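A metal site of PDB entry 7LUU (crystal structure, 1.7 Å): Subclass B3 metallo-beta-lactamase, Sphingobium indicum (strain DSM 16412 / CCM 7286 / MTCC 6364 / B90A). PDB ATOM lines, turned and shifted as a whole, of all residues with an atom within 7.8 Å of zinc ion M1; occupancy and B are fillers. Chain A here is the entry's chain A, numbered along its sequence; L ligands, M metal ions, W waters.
NE2 of His 127 binds zinc ion M1, at 2.0 Å.
Zinc ion M1 is bound by a ring nitrogen (NE2) of His 267, at 2.0 Å.
Zinc ion M1 is bound by water W2.
The side-chain carboxylate (OD2) of Asp 126 binds zinc ion M1, 2.1 Å away.
An oxygen (O2) of the ligand binds zinc ion M1 (2.1 Å).
Water W1 binds zinc ion M1, 2.3 Å away.
Three residues have an atom within 4 Å of zinc ion M1: Asp 126, His 127 and His 267.
The nearest printed residue that does not touch zinc ion M1 is Glu 122 (4.2 Å).
Water W2 bridges OE1 of Glu 122 (3.0 Å) and OG of Ser 225 (3.3 Å).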
ATOM      1  N   TRP A  55     -21.405  16.775   8.158  1.00  0.00           N
ATOM      2  CA  TRP A  55     -20.710  16.494   6.901  1.00  0.00           C
ATOM      3  C   TRP A  55     -20.547  14.994   6.682  1.00  0.00           C
ATOM      4  O   TRP A  55     -20.668  14.533   5.548  1.00  0.00           O
ATOM      5  CB  TRP A  55     -19.300  17.099   6.900  1.00  0.00           C
ATOM      6  CG  TRP A  55     -19.207  18.530   6.544  1.00  0.00           C
ATOM      7  CD1 TRP A  55     -20.053  19.251   5.748  1.00  0.00           C
ATOM      8  CD2 TRP A  55     -18.143  19.420   6.929  1.00  0.00           C
ATOM      9  NE1 TRP A  55     -19.568  20.568   5.625  1.00  0.00           N
ATOM     10  CE2 TRP A  55     -18.400  20.673   6.351  1.00  0.00           C
ATOM     11  CE3 TRP A  55     -16.997  19.261   7.731  1.00  0.00           C
ATOM     12  CZ2 TRP A  55     -17.538  21.772   6.543  1.00  0.00           C
ATOM     13  CZ3 TRP A  55     -16.158  20.364   7.952  1.00  0.00           C
ATOM     14  CH2 TRP A  55     -16.435  21.592   7.335  1.00  0.00           C
ATOM     15  N   GLY A  75     -22.993  15.068   3.619  1.00  0.00           N
ATOM     16  CA  GLY A  75     -22.617  16.453   3.341  1.00  0.00           C
ATOM     17  C   GLY A  75     -21.374  16.646   2.461  1.00  0.00           C
ATOM     18  O   GLY A  75     -21.018  17.805   2.152  1.00  0.00           O
ATOM     19  N   LEU A  76     -20.742  15.552   2.019  1.00  0.00           N
ATOM     20  CA  LEU A  76     -19.496  15.654   1.216  1.00  0.00           C
ATOM     21  C   LEU A  76     -19.502  14.518   0.232  1.00  0.00           C
ATOM     22  O   LEU A  76     -19.536  13.337   0.622  1.00  0.00           O
ATOM     23  CB  LEU A  76     -18.249  15.558   2.145  1.00  0.00           C
ATOM     24  CG  LEU A  76     -18.060  16.710   3.146  1.00  0.00           C
ATOM     25  CD1 LEU A  76     -16.987  16.403   4.178  1.00  0.00           C
ATOM     26  CD2 LEU A  76     -17.699  17.979   2.360  1.00  0.00           C
ATOM     27  N   THR A 121     -10.824  18.089  -6.215  1.00  0.00           N
ATOM     28  CA  THR A 121     -11.484  19.290  -6.715  1.00  0.00           C
ATOM     29  C   THR A 121     -10.889  20.564  -6.138  1.00  0.00           C
ATOM     30  O   THR A 121     -11.031  21.643  -6.758  1.00  0.00           O
ATOM     31  CB  THR A 121     -13.010  19.277  -6.413  1.00  0.00           C
ATOM     32  OG1 THR A 121     -13.285  19.171  -5.005  1.00  0.00           O
ATOM     33  CG2 THR A 121     -13.733  18.127  -7.206  1.00  0.00           C
ATOM     34  N   GLU A 122     -10.359  20.495  -4.908  1.00  0.00           N
ATOM     35  CA  GLU A 122      -9.838  21.699  -4.236  1.00  0.00           C
ATOM     36  C   GLU A 122      -9.009  21.353  -3.007  1.00  0.00           C
ATOM     37  O   GLU A 122      -9.277  20.351  -2.312  1.00  0.00           O
ATOM     38  CB  GLU A 122     -10.963  22.659  -3.808  1.00  0.00           C
ATOM     39  CG  GLU A 122     -11.955  21.981  -2.769  1.00  0.00           C
ATOM     40  CD  GLU A 122     -12.909  23.000  -2.156  1.00  0.00           C
ATOM     41  OE1 GLU A 122     -14.038  23.145  -2.709  1.00  0.00           O
ATOM     42  OE2 GLU A 122     -12.578  23.592  -1.124  1.00  0.00           O
ATOM     43  N   HIS A 124      -8.799  22.145   0.175  1.00  0.00           N
ATOM     44  CA  HIS A 124      -9.309  22.534   1.470  1.00  0.00           C
ATOM     45  C   HIS A 124      -9.579  21.254   2.248  1.00  0.00           C
ATOM     46  O   HIS A 124      -9.819  20.181   1.648  1.00  0.00           O
ATOM     47  CB  HIS A 124     -10.609  23.299   1.326  1.00  0.00           C
ATOM     48  CG  HIS A 124     -10.425  24.730   0.942  1.00  0.00           C
ATOM     49  ND1 HIS A 124     -11.487  25.550   0.652  1.00  0.00           N
ATOM     50  CD2 HIS A 124      -9.302  25.497   0.861  1.00  0.00           C
ATOM     51  CE1 HIS A 124     -11.020  26.781   0.394  1.00  0.00           C
ATOM     52  NE2 HIS A 124      -9.706  26.776   0.522  1.00  0.00           N
ATOM     53  N   TYR A 125      -9.507  21.352   3.588  1.00  0.00           N
ATOM     54  CA  TYR A 125      -9.487  20.091   4.349  1.00  0.00           C
ATOM     55  C   TYR A 125     -10.808  19.304   4.318  1.00  0.00           C
ATOM     56  O   TYR A 125     -10.786  18.108   4.642  1.00  0.00           O
ATOM     57  CB  TYR A 125      -9.028  20.397   5.803  1.00  0.00           C
ATOM     58  CG  TYR A 125     -10.042  21.135   6.658  1.00  0.00           C
ATOM     59  CD1 TYR A 125     -11.155  20.474   7.143  1.00  0.00           C
ATOM     60  CD2 TYR A 125      -9.867  22.482   7.009  1.00  0.00           C
ATOM     61  CE1 TYR A 125     -12.062  21.088   7.948  1.00  0.00           C
ATOM     62  CE2 TYR A 125     -10.766  23.114   7.844  1.00  0.00           C
ATOM     63  CZ  TYR A 125     -11.876  22.412   8.280  1.00  0.00           C
ATOM     64  OH  TYR A 125     -12.796  23.025   9.105  1.00  0.00           O
ATOM     65  N   ASP A 126     -11.943  19.910   3.907  1.00  0.00           N
ATOM     66  CA  ASP A 126     -13.175  19.130   3.854  1.00  0.00           C
ATOM     67  C   ASP A 126     -13.295  18.364   2.547  1.00  0.00           C
ATOM     68  O   ASP A 126     -14.223  17.570   2.399  1.00  0.00           O
ATOM     69  CB  ASP A 126     -14.434  20.027   4.072  1.00  0.00           C
ATOM     70  CG  ASP A 126     -14.504  21.241   3.100  1.00  0.00           C
ATOM     71  OD1 ASP A 126     -13.458  21.847   2.764  1.00  0.00           O
ATOM     72  OD2 ASP A 126     -15.640  21.624   2.738  1.00  0.00           O
ATOM     73  N   HIS A 127     -12.358  18.532   1.588  1.00  0.00           N
ATOM     74  CA  HIS A 127     -12.335  17.722   0.379  1.00  0.00           C
ATOM     75  C   HIS A 127     -11.017  17.026   0.181  1.00  0.00           C
ATOM     76  O   HIS A 127     -10.979  15.953  -0.402  1.00  0.00           O
ATOM     77  CB  HIS A 127     -12.632  18.598  -0.880  1.00  0.00           C
ATOM     78  CG  HIS A 127     -13.839  19.469  -0.692  1.00  0.00           C
ATOM     79  ND1 HIS A 127     -15.116  18.998  -0.951  1.00  0.00           N
ATOM     80  CD2 HIS A 127     -13.984  20.703  -0.166  1.00  0.00           C
ATOM     81  CE1 HIS A 127     -16.004  19.928  -0.599  1.00  0.00           C
ATOM     82  NE2 HIS A 127     -15.338  20.972  -0.133  1.00  0.00           N
ATOM     83  N   GLN A 163      -9.962  32.121   1.729  1.00  0.00           N
ATOM     84  CA  GLN A 163     -10.040  31.667   3.107  1.00  0.00           C
ATOM     85  C   GLN A 163      -8.658  31.601   3.759  1.00  0.00           C
ATOM     86  O   GLN A 163      -8.527  31.013   4.833  1.00  0.00           O
ATOM     87  CB  GLN A 163     -10.736  30.304   3.200  1.00  0.00           C
ATOM     88  CG  GLN A 163     -12.205  30.391   2.787  1.00  0.00           C
ATOM     89  CD  GLN A 163     -12.928  29.089   2.890  1.00  0.00           C
ATOM     90  OE1 GLN A 163     -13.465  28.545   1.887  1.00  0.00           O
ATOM     91  NE2 GLN A 163     -12.989  28.580   4.103  1.00  0.00           N
ATOM     92  N   HIS A 200     -13.768  29.557  -6.049  1.00  0.00           N
ATOM     93  CA  HIS A 200     -13.729  29.223  -4.624  1.00  0.00           C
ATOM     94  C   HIS A 200     -12.280  29.223  -4.141  1.00  0.00           C
ATOM     95  O   HIS A 200     -11.956  29.762  -3.057  1.00  0.00           O
ATOM     96  CB  HIS A 200     -14.414  27.860  -4.448  1.00  0.00           C
ATOM     97  CG  HIS A 200     -14.432  27.368  -3.036  1.00  0.00           C
ATOM     98  ND1 HIS A 200     -15.273  27.883  -2.067  1.00  0.00           N
ATOM     99  CD2 HIS A 200     -13.682  26.407  -2.437  1.00  0.00           C
ATOM    100  CE1 HIS A 200     -15.030  27.267  -0.907  1.00  0.00           C
ATOM    101  NE2 HIS A 200     -14.088  26.352  -1.117  1.00  0.00           N
ATOM    102  N   SER A 225     -16.889  22.859  -5.740  1.00  0.00           N
ATOM    103  CA  SER A 225     -17.590  24.007  -5.180  1.00  0.00           C
ATOM    104  C   SER A 225     -17.342  25.250  -6.015  1.00  0.00           C
ATOM    105  O   SER A 225     -16.216  25.524  -6.406  1.00  0.00           O
ATOM    106  CB  SER A 225     -17.142  24.229  -3.763  1.00  0.00           C
ATOM    107  OG  SER A 225     -17.803  25.396  -3.229  1.00  0.00           O
ATOM    108  N   ASN A 227     -18.692  28.094  -4.409  1.00  0.00           N
ATOM    109  CA  ASN A 227     -19.316  28.992  -3.416  1.00  0.00           C
ATOM    110  C   ASN A 227     -18.374  30.145  -3.127  1.00  0.00           C
ATOM    111  O   ASN A 227     -17.227  29.919  -2.753  1.00  0.00           O
ATOM    112  CB  ASN A 227     -19.624  28.242  -2.136  1.00  0.00           C
ATOM    113  CG  ASN A 227     -20.638  27.212  -2.370  1.00  0.00           C
ATOM    114  OD1 ASN A 227     -21.557  27.403  -3.197  1.00  0.00           O
ATOM    115  ND2 ASN A 227     -20.509  26.099  -1.670  1.00  0.00           N
ATOM    116  N   VAL A 229     -17.060  32.099  -0.784  1.00  0.00           N
ATOM    117  CA  VAL A 229     -16.931  32.320   0.651  1.00  0.00           C
ATOM    118  C   VAL A 229     -15.490  32.668   0.966  1.00  0.00           C
ATOM    119  O   VAL A 229     -14.558  32.407   0.192  1.00  0.00           O
ATOM    120  CB  VAL A 229     -17.417  31.113   1.452  1.00  0.00           C
ATOM    121  CG1 VAL A 229     -18.907  31.004   1.278  1.00  0.00           C
ATOM    122  CG2 VAL A 229     -16.733  29.906   0.972  1.00  0.00           C
ATOM    123  N   ALA A 266     -19.553  18.735  -5.134  1.00  0.00           N
ATOM    124  CA  ALA A 266     -18.674  18.415  -3.983  1.00  0.00           C
ATOM    125  C   ALA A 266     -19.406  18.528  -2.616  1.00  0.00           C
ATOM    126  O   ALA A 266     -19.311  17.626  -1.787  1.00  0.00           O
ATOM    127  CB  ALA A 266     -17.478  19.357  -3.976  1.00  0.00           C
ATOM    128  N   HIS A 267     -20.144  19.617  -2.382  1.00  0.00           N
ATOM    129  CA  HIS A 267     -21.143  19.613  -1.314  1.00  0.00           C
ATOM    130  C   HIS A 267     -22.486  19.276  -1.959  1.00  0.00           C
ATOM    131  O   HIS A 267     -23.010  20.126  -2.696  1.00  0.00           O
ATOM    132  CB  HIS A 267     -21.226  21.028  -0.692  1.00  0.00           C
ATOM    133  CG  HIS A 267     -20.000  21.379   0.116  1.00  0.00           C
ATOM    134  ND1 HIS A 267     -19.897  21.053   1.457  1.00  0.00           N
ATOM    135  CD2 HIS A 267     -18.841  21.975  -0.227  1.00  0.00           C
ATOM    136  CE1 HIS A 267     -18.737  21.465   1.905  1.00  0.00           C
ATOM    137  NE2 HIS A 267     -18.046  21.997   0.898  1.00  0.00           N
ATOM    138  N   ASN A 270     -25.515  21.770  -2.421  1.00  0.00           N
ATOM    139  CA  ASN A 270     -25.466  22.880  -3.376  1.00  0.00           C
ATOM    140  C   ASN A 270     -26.231  22.571  -4.642  1.00  0.00           C
ATOM    141  O   ASN A 270     -26.649  23.509  -5.356  1.00  0.00           O
ATOM    142  CB  ASN A 270     -24.010  23.193  -3.810  1.00  0.00           C
ATOM    143  CG  ASN A 270     -23.130  23.713  -2.676  1.00  0.00           C
ATOM    144  OD1 ASN A 270     -21.914  23.931  -2.895  1.00  0.00           O
ATOM    145  ND2 ASN A 270     -23.706  23.917  -1.490  1.00  0.00           N
HETATM  146  C1  LIG L   1     -18.394  25.699   0.969  1.00  0.00           C
HETATM  147  O1  LIG L   1     -17.782  25.715  -0.236  1.00  0.00           O
HETATM  148  C2  LIG L   1     -17.401  25.467   2.000  1.00  0.00           C
HETATM  149  O2  LIG L   1     -16.802  24.195   2.028  1.00  0.00           O
HETATM  150  C3  LIG L   1     -16.421  26.670   2.065  1.00  0.00           C
HETATM  151  O3  LIG L   1     -15.145  26.142   2.358  1.00  0.00           O
HETATM  152 ZN    ZN M   1     -16.081  22.535   0.910  1.00  0.00          ZN
HETATM  153 ZN    ZN M   2     -13.319  24.912   0.043  1.00  0.00          ZN
HETATM  154  O   HOH W   1     -14.301  23.850   1.333  1.00  0.00           O
HETATM  155  O   HOH W   2     -16.312  23.732  -0.764  1.00  0.00           O
